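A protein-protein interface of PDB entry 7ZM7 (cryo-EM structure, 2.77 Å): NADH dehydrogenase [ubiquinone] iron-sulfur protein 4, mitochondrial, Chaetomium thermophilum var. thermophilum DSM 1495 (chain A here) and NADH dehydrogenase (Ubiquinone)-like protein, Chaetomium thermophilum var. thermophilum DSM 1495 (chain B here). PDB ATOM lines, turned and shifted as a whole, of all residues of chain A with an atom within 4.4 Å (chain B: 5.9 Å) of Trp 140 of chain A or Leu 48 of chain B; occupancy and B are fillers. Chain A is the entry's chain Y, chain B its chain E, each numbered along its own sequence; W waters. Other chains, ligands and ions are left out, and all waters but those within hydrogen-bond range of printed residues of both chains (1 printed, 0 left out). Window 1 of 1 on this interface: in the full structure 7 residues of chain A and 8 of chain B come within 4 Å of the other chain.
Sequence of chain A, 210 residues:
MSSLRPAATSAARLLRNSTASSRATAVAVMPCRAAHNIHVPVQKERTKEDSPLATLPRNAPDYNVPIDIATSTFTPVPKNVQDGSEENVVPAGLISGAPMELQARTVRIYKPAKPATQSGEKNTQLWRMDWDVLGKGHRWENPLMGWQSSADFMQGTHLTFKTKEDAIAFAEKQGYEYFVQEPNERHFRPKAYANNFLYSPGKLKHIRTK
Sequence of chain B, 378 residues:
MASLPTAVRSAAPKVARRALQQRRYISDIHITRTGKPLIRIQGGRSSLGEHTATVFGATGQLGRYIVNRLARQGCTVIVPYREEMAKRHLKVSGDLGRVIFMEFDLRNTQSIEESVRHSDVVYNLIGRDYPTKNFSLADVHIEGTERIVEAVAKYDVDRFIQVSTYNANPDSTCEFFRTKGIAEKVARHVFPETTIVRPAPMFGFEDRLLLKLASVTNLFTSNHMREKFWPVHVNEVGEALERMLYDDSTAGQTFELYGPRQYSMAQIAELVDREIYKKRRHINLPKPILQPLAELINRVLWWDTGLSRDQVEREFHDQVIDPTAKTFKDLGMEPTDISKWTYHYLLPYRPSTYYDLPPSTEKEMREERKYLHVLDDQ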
ATOM      1  N   GLY A 137     -12.540  21.227 -11.912  1.00  0.00           N
ATOM      2  CA  GLY A 137     -11.237  20.632 -11.575  1.00  0.00           C
ATOM      3  C   GLY A 137     -10.606  21.222 -10.347  1.00  0.00           C
ATOM      4  O   GLY A 137      -9.563  20.716  -9.960  1.00  0.00           O
ATOM      5  N   ARG A 139     -12.104  21.722  -7.097  1.00  0.00           N
ATOM      6  CA  ARG A 139     -12.466  20.908  -5.943  1.00  0.00           C
ATOM      7  C   ARG A 139     -13.667  20.064  -6.303  1.00  0.00           C
ATOM      8  O   ARG A 139     -14.628  20.569  -6.875  1.00  0.00           O
ATOM      9  CB  ARG A 139     -12.814  21.750  -4.713  1.00  0.00           C
ATOM     10  CG  ARG A 139     -11.672  22.376  -4.018  1.00  0.00           C
ATOM     11  CD  ARG A 139     -10.705  21.373  -3.525  1.00  0.00           C
ATOM     12  NE  ARG A 139      -9.674  22.052  -2.760  1.00  0.00           N
ATOM     13  CZ  ARG A 139      -8.608  22.636  -3.288  1.00  0.00           C
ATOM     14  NH1 ARG A 139      -7.746  23.235  -2.497  1.00  0.00           N
ATOM     15  NH2 ARG A 139      -8.390  22.590  -4.586  1.00  0.00           N
ATOM     16  N   TRP A 140     -13.618  18.793  -5.951  1.00  0.00           N
ATOM     17  CA  TRP A 140     -14.820  17.986  -5.941  1.00  0.00           C
ATOM     18  C   TRP A 140     -14.793  17.112  -4.710  1.00  0.00           C
ATOM     19  O   TRP A 140     -13.762  16.937  -4.071  1.00  0.00           O
ATOM     20  CB  TRP A 140     -14.990  17.163  -7.218  1.00  0.00           C
ATOM     21  CG  TRP A 140     -13.960  16.142  -7.494  1.00  0.00           C
ATOM     22  CD1 TRP A 140     -13.966  14.846  -7.093  1.00  0.00           C
ATOM     23  CD2 TRP A 140     -12.782  16.311  -8.278  1.00  0.00           C
ATOM     24  NE1 TRP A 140     -12.862  14.202  -7.560  1.00  0.00           N
ATOM     25  CE2 TRP A 140     -12.115  15.081  -8.292  1.00  0.00           C
ATOM     26  CE3 TRP A 140     -12.215  17.388  -8.951  1.00  0.00           C
ATOM     27  CZ2 TRP A 140     -10.923  14.897  -8.950  1.00  0.00           C
ATOM     28  CZ3 TRP A 140     -11.034  17.204  -9.594  1.00  0.00           C
ATOM     29  CH2 TRP A 140     -10.398  15.968  -9.598  1.00  0.00           C
ATOM     30  N   GLU A 141     -15.959  16.594  -4.373  1.00  0.00           N
ATOM     31  CA  GLU A 141     -16.128  15.780  -3.186  1.00  0.00           C
ATOM     32  C   GLU A 141     -15.695  14.353  -3.464  1.00  0.00           C
ATOM     33  O   GLU A 141     -16.110  13.754  -4.454  1.00  0.00           O
ATOM     34  CB  GLU A 141     -17.585  15.806  -2.757  1.00  0.00           C
ATOM     35  CG  GLU A 141     -17.845  15.319  -1.377  1.00  0.00           C
ATOM     36  CD  GLU A 141     -19.222  14.718  -1.271  1.00  0.00           C
ATOM     37  OE1 GLU A 141     -19.731  14.255  -2.308  1.00  0.00           O
ATOM     38  OE2 GLU A 141     -19.803  14.711  -0.167  1.00  0.00           O
ATOM     39  N   ASN A 142     -14.859  13.817  -2.596  1.00  0.00           N
ATOM     40  CA  ASN A 142     -14.481  12.412  -2.676  1.00  0.00           C
ATOM     41  C   ASN A 142     -15.685  11.542  -2.337  1.00  0.00           C
ATOM     42  O   ASN A 142     -16.295  11.728  -1.287  1.00  0.00           O
ATOM     43  CB  ASN A 142     -13.335  12.138  -1.703  1.00  0.00           C
ATOM     44  CG  ASN A 142     -12.905  10.698  -1.673  1.00  0.00           C
ATOM     45  OD1 ASN A 142     -13.029   9.963  -2.642  1.00  0.00           O
ATOM     46  ND2 ASN A 142     -12.433  10.272  -0.522  1.00  0.00           N
ATOM     47  N   PRO A 143     -16.052  10.590  -3.188  1.00  0.00           N
ATOM     48  CA  PRO A 143     -17.205   9.736  -2.862  1.00  0.00           C
ATOM     49  C   PRO A 143     -17.014   8.903  -1.610  1.00  0.00           C
ATOM     50  O   PRO A 143     -17.994   8.611  -0.924  1.00  0.00           O
ATOM     51  CB  PRO A 143     -17.346   8.849  -4.107  1.00  0.00           C
ATOM     52  CG  PRO A 143     -16.535   9.472  -5.133  1.00  0.00           C
ATOM     53  CD  PRO A 143     -15.466  10.246  -4.488  1.00  0.00           C
ATOM     54  N   TRP A 147     -13.740  13.734   1.425  1.00  0.00           N
ATOM     55  CA  TRP A 147     -12.609  14.681   1.268  1.00  0.00           C
ATOM     56  C   TRP A 147     -12.758  15.487  -0.015  1.00  0.00           C
ATOM     57  O   TRP A 147     -13.550  15.104  -0.874  1.00  0.00           O
ATOM     58  CB  TRP A 147     -11.258  13.974   1.270  1.00  0.00           C
ATOM     59  CG  TRP A 147     -10.941  13.226   2.524  1.00  0.00           C
ATOM     60  CD1 TRP A 147     -11.401  13.469   3.784  1.00  0.00           C
ATOM     61  CD2 TRP A 147     -10.057  12.101   2.624  1.00  0.00           C
ATOM     62  NE1 TRP A 147     -10.875  12.558   4.659  1.00  0.00           N
ATOM     63  CE2 TRP A 147     -10.044  11.712   3.976  1.00  0.00           C
ATOM     64  CE3 TRP A 147      -9.293  11.385   1.699  1.00  0.00           C
ATOM     65  CZ2 TRP A 147      -9.285  10.636   4.427  1.00  0.00           C
ATOM     66  CZ3 TRP A 147      -8.544  10.322   2.145  1.00  0.00           C
ATOM     67  CH2 TRP A 147      -8.549   9.956   3.488  1.00  0.00           C
ATOM     68  N   GLN A 148     -12.015  16.584  -0.117  1.00  0.00           N
ATOM     69  CA  GLN A 148     -12.064  17.418  -1.331  1.00  0.00           C
ATOM     70  C   GLN A 148     -10.884  17.064  -2.233  1.00  0.00           C
ATOM     71  O   GLN A 148      -9.747  17.355  -1.852  1.00  0.00           O
ATOM     72  CB  GLN A 148     -12.139  18.881  -0.927  1.00  0.00           C
ATOM     73  CG  GLN A 148     -13.248  19.153   0.077  1.00  0.00           C
ATOM     74  CD  GLN A 148     -13.436  20.624   0.336  1.00  0.00           C
ATOM     75  OE1 GLN A 148     -14.170  21.306  -0.374  1.00  0.00           O
ATOM     76  NE2 GLN A 148     -12.774  21.126   1.365  1.00  0.00           N
ATOM     77  N   SER A 149     -11.236  16.492  -3.437  1.00  0.00           N
ATOM     78  CA  SER A 149     -10.210  16.126  -4.446  1.00  0.00           C
ATOM     79  C   SER A 149      -9.971  17.292  -5.407  1.00  0.00           C
ATOM     80  O   SER A 149     -10.852  18.147  -5.508  1.00  0.00           O
ATOM     81  CB  SER A 149     -10.638  14.905  -5.185  1.00  0.00           C
ATOM     82  OG  SER A 149     -11.341  14.018  -4.333  1.00  0.00           O
ATOM     83  N   SER A 150      -8.777  17.325  -6.057  1.00  0.00           N
ATOM     84  CA  SER A 150      -8.474  18.425  -7.009  1.00  0.00           C
ATOM     85  C   SER A 150      -7.712  17.942  -8.238  1.00  0.00           C
ATOM     86  O   SER A 150      -7.095  16.875  -8.173  1.00  0.00           O
ATOM     87  CB  SER A 150      -7.686  19.508  -6.344  1.00  0.00           C
ATOM     88  OG  SER A 150      -7.543  20.639  -7.185  1.00  0.00           O
ATOM     89  N   ALA A 151      -7.778  18.706  -9.321  1.00  0.00           N
ATOM     90  CA  ALA A 151      -6.976  18.418 -10.526  1.00  0.00           C
ATOM     91  C   ALA A 151      -6.061  19.618 -10.747  1.00  0.00           C
ATOM     92  O   ALA A 151      -5.233  19.572 -11.652  1.00  0.00           O
ATOM     93  CB  ALA A 151      -7.905  18.295 -11.687  1.00  0.00           C
ATOM     94  N   ILE B  39     -24.088  13.578 -12.522  1.00  0.00           N
ATOM     95  CA  ILE B  39     -23.256  14.719 -12.891  1.00  0.00           C
ATOM     96  C   ILE B  39     -21.803  14.305 -12.760  1.00  0.00           C
ATOM     97  O   ILE B  39     -21.207  14.434 -11.688  1.00  0.00           O
ATOM     98  CB  ILE B  39     -23.530  15.959 -12.026  1.00  0.00           C
ATOM     99  CG1 ILE B  39     -24.963  16.438 -12.196  1.00  0.00           C
ATOM    100  CG2 ILE B  39     -22.636  17.082 -12.464  1.00  0.00           C
ATOM    101  CD1 ILE B  39     -25.940  15.797 -11.243  1.00  0.00           C
ATOM    102  N   ARG B  40     -21.218  13.834 -13.844  1.00  0.00           N
ATOM    103  CA  ARG B  40     -19.873  13.298 -13.804  1.00  0.00           C
ATOM    104  C   ARG B  40     -18.829  14.387 -14.010  1.00  0.00           C
ATOM    105  O   ARG B  40     -19.061  15.387 -14.691  1.00  0.00           O
ATOM    106  CB  ARG B  40     -19.706  12.211 -14.861  1.00  0.00           C
ATOM    107  CG  ARG B  40     -19.481  12.716 -16.254  1.00  0.00           C
ATOM    108  CD  ARG B  40     -19.461  11.600 -17.271  1.00  0.00           C
ATOM    109  NE  ARG B  40     -20.797  11.119 -17.584  1.00  0.00           N
ATOM    110  CZ  ARG B  40     -21.073  10.234 -18.535  1.00  0.00           C
ATOM    111  NH1 ARG B  40     -22.321   9.856 -18.735  1.00  0.00           N
ATOM    112  NH2 ARG B  40     -20.108   9.736 -19.291  1.00  0.00           N
ATOM    113  N   ILE B  41     -17.677  14.186 -13.385  1.00  0.00           N
ATOM    114  CA  ILE B  41     -16.466  14.951 -13.645  1.00  0.00           C
ATOM    115  C   ILE B  41     -15.507  14.013 -14.351  1.00  0.00           C
ATOM    116  O   ILE B  41     -15.147  12.965 -13.811  1.00  0.00           O
ATOM    117  CB  ILE B  41     -15.863  15.502 -12.345  1.00  0.00           C
ATOM    118  CG1 ILE B  41     -16.828  16.495 -11.703  1.00  0.00           C
ATOM    119  CG2 ILE B  41     -14.499  16.123 -12.592  1.00  0.00           C
ATOM    120  CD1 ILE B  41     -16.650  16.661 -10.252  1.00  0.00           C
ATOM    121  N   GLN B  42     -15.098  14.376 -15.555  1.00  0.00           N
ATOM    122  CA  GLN B  42     -14.395  13.455 -16.439  1.00  0.00           C
ATOM    123  C   GLN B  42     -12.898  13.631 -16.277  1.00  0.00           C
ATOM    124  O   GLN B  42     -12.298  14.527 -16.862  1.00  0.00           O
ATOM    125  CB  GLN B  42     -14.816  13.684 -17.879  1.00  0.00           C
ATOM    126  CG  GLN B  42     -16.247  13.327 -18.110  1.00  0.00           C
ATOM    127  CD  GLN B  42     -16.675  13.564 -19.512  1.00  0.00           C
ATOM    128  OE1 GLN B  42     -15.912  14.062 -20.331  1.00  0.00           O
ATOM    129  NE2 GLN B  42     -17.902  13.198 -19.815  1.00  0.00           N
ATOM    130  N   GLY B  43     -12.294  12.764 -15.488  1.00  0.00           N
ATOM    131  CA  GLY B  43     -10.861  12.734 -15.358  1.00  0.00           C
ATOM    132  C   GLY B  43     -10.356  11.314 -15.302  1.00  0.00           C
ATOM    133  O   GLY B  43     -10.750  10.478 -16.113  1.00  0.00           O
ATOM    134  N   GLY B  44      -9.499  11.026 -14.338  1.00  0.00           N
ATOM    135  CA  GLY B  44      -8.922   9.711 -14.216  1.00  0.00           C
ATOM    136  C   GLY B  44      -9.327   9.001 -12.950  1.00  0.00           C
ATOM    137  O   GLY B  44     -10.514   8.886 -12.645  1.00  0.00           O
ATOM    138  N   SER B  46      -9.049   9.524  -9.575  1.00  0.00           N
ATOM    139  CA  SER B  46      -9.712  10.208  -8.434  1.00  0.00           C
ATOM    140  C   SER B  46     -10.984  10.914  -8.891  1.00  0.00           C
ATOM    141  O   SER B  46     -11.639  11.521  -8.040  1.00  0.00           O
ATOM    142  CB  SER B  46      -8.781  11.164  -7.739  1.00  0.00           C
ATOM    143  OG  SER B  46      -7.457  10.657  -7.727  1.00  0.00           O
ATOM    144  N   SER B  47     -11.316  10.838 -10.175  1.00  0.00           N
ATOM    145  CA  SER B  47     -12.486  11.577 -10.716  1.00  0.00           C
ATOM    146  C   SER B  47     -13.836  11.004 -10.282  1.00  0.00           C
ATOM    147  O   SER B  47     -13.873  10.210  -9.374  1.00  0.00           O
ATOM    148  CB  SER B  47     -12.406  11.664 -12.204  1.00  0.00           C
ATOM    149  OG  SER B  47     -12.710  10.416 -12.805  1.00  0.00           O
ATOM    150  N   LEU B  48     -14.924  11.429 -10.912  1.00  0.00           N
ATOM    151  CA  LEU B  48     -16.290  11.019 -10.599  1.00  0.00           C
ATOM    152  C   LEU B  48     -16.957  10.574 -11.891  1.00  0.00           C
ATOM    153  O   LEU B  48     -17.538  11.386 -12.605  1.00  0.00           O
ATOM    154  CB  LEU B  48     -17.069  12.168  -9.944  1.00  0.00           C
ATOM    155  CG  LEU B  48     -16.493  12.830  -8.694  1.00  0.00           C
ATOM    156  CD1 LEU B  48     -17.482  13.767  -8.087  1.00  0.00           C
ATOM    157  CD2 LEU B  48     -16.079  11.798  -7.690  1.00  0.00           C
ATOM    158  N   GLY B  49     -16.880   9.281 -12.193  1.00  0.00           N
ATOM    159  CA  GLY B  49     -17.643   8.752 -13.307  1.00  0.00           C
ATOM    160  C   GLY B  49     -19.114   8.577 -12.981  1.00  0.00           C
ATOM    161  O   GLY B  49     -19.968   8.669 -13.865  1.00  0.00           O
ATOM    162  N   GLU B  50     -19.424   8.299 -11.717  1.00  0.00           N
ATOM    163  CA  GLU B  50     -20.777   8.239 -11.174  1.00  0.00           C
ATOM    164  C   GLU B  50     -21.606   7.079 -11.714  1.00  0.00           C
ATOM    165  O   GLU B  50     -22.730   6.849 -11.266  1.00  0.00           O
ATOM    166  CB  GLU B  50     -21.496   9.568 -11.395  1.00  0.00           C
ATOM    167  CG  GLU B  50     -22.758   9.724 -10.585  1.00  0.00           C
ATOM    168  CD  GLU B  50     -22.572   9.403  -9.109  1.00  0.00           C
ATOM    169  OE1 GLU B  50     -21.504   9.709  -8.545  1.00  0.00           O
ATOM    170  OE2 GLU B  50     -23.504   8.831  -8.508  1.00  0.00           O
ATOM    171  N   GLN B  73     -11.607   5.476 -14.876  1.00  0.00           N
ATOM    172  CA  GLN B  73     -12.256   6.759 -15.107  1.00  0.00           C
ATOM    173  C   GLN B  73     -13.214   7.145 -13.983  1.00  0.00           C
ATOM    174  O   GLN B  73     -14.083   7.991 -14.195  1.00  0.00           O
ATOM    175  CB  GLN B  73     -12.994   6.746 -16.438  1.00  0.00           C
ATOM    176  CG  GLN B  73     -14.135   5.774 -16.461  1.00  0.00           C
ATOM    177  CD  GLN B  73     -14.842   5.693 -17.789  1.00  0.00           C
ATOM    178  OE1 GLN B  73     -15.767   4.899 -17.973  1.00  0.00           O
ATOM    179  NE2 GLN B  73     -14.422   6.532 -18.721  1.00  0.00           N
ATOM    180  N   GLY B  74     -13.090   6.536 -12.810  1.00  0.00           N
ATOM    181  CA  GLY B  74     -13.786   7.004 -11.631  1.00  0.00           C
ATOM    182  C   GLY B  74     -15.138   6.400 -11.343  1.00  0.00           C
ATOM    183  O   GLY B  74     -15.952   7.048 -10.684  1.00  0.00           O
ATOM    184  N   CYS B  75     -15.409   5.183 -11.800  1.00  0.00           N
ATOM    185  CA  CYS B  75     -16.705   4.553 -11.614  1.00  0.00           C
ATOM    186  C   CYS B  75     -16.590   3.400 -10.633  1.00  0.00           C
ATOM    187  O   CYS B  75     -15.564   2.723 -10.591  1.00  0.00           O
ATOM    188  CB  CYS B  75     -17.259   4.043 -12.943  1.00  0.00           C
ATOM    189  SG  CYS B  75     -17.319   5.258 -14.267  1.00  0.00           S
ATOM    190  N   ARG B  98     -13.692   1.958  -5.051  1.00  0.00           N
ATOM    191  CA  ARG B  98     -14.182   1.855  -6.446  1.00  0.00           C
ATOM    192  C   ARG B  98     -14.379   0.397  -6.866  1.00  0.00           C
ATOM    193  O   ARG B  98     -15.480   0.082  -7.322  1.00  0.00           O
ATOM    194  CB  ARG B  98     -13.296   2.685  -7.376  1.00  0.00           C
ATOM    195  CG  ARG B  98     -13.360   4.184  -7.131  1.00  0.00           C
ATOM    196  CD  ARG B  98     -14.804   4.606  -6.974  1.00  0.00           C
ATOM    197  NE  ARG B  98     -15.042   5.943  -7.483  1.00  0.00           N
ATOM    198  CZ  ARG B  98     -16.228   6.529  -7.495  1.00  0.00           C
ATOM    199  NH1 ARG B  98     -16.356   7.749  -7.984  1.00  0.00           N
ATOM    200  NH2 ARG B  98     -17.279   5.892  -7.016  1.00  0.00           N
HETATM  201  O   HOH W   1     -12.269  11.458  -5.496  1.00  0.00           O
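Water W1 lies within hydrogen-bond range of O of Ser 46 of chain B (2.6 Å), OG of Ser 149 of chain A (3.0 Å), OD1 of Asn 142 of chain A (3.3 Å) and NE1 of Trp 140 of chain A (3.5 Å).
Trp 140 of chain A touches just these residues of chain B: Ile 41, Ser 46 and Leu 48.
Leu 48 of chain B touches just these residues of chain A: Trp 140 (3.6 Å), Glu 141 (3.8 Å) and Pro 143 (3.5 Å).
Printed residues of chain A within 4 Å of Ile 41 of chain B: Trp 140.
Of the printed residues of chain A, Ser 46 of chain B touches Trp 140.
Printed residues of chain A within 4 Å of Arg 98 of chain B: Pro 143 (3.3 Å).
Gln 73 of chain B touches none of the printed residues of chain A.
The nearest printed residue of chain A that does not touch Ile 41 of chain B is Gly 137 of chain A (5.5 Å).
Hydrophobic or aromatic side chains of chain B that line the printed part of chain A: Ile 41 and Leu 48.
Printed residues of chain A that touch a printed residue of chain B: Trp 140, Glu 141 and Pro 143.
Hydrophobic or aromatic side chains of chain A that line the printed part of chain B: Trp 140 and Pro 143.
Among the printed residues, 6 pairs touch across the chains.
Among the printed residues, no Asp or Glu carboxylate lies within 4 Å of a Lys or Arg side-chain nitrogen of the other chain.
N of Ile 41 of chain B is in hydrogen-bond range of O of Leu 48 of chain B (2.9 Å).
NH1 of Arg 98 of chain B is in hydrogen-bond range of O of Gly 74 of chain B, 2.8 Å away.
The backbone carbonyl oxygen of Trp 140 of chain A lies within hydrogen-bond range of the backbone NH of Ser 149 of chain A, 2.6 Å away.
Among the printed residues, pairs that only touch across the chains: Trp 140 of chain A with Ile 41 of chain B, Trp 140 of chain A with Leu 48 of chain B, Glu 141 of chain A with Leu 48 of chain B, Pro 143 of chain A with Leu 48 of chain B and Pro 143 of chain A with Arg 98 of chain B.
The backbone carbonyl oxygen (O) of Ser 46 of chain B is in hydrogen-bond range of the indole nitrogen (NE1) of Trp 140 of chain A, 3.0 Å away.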
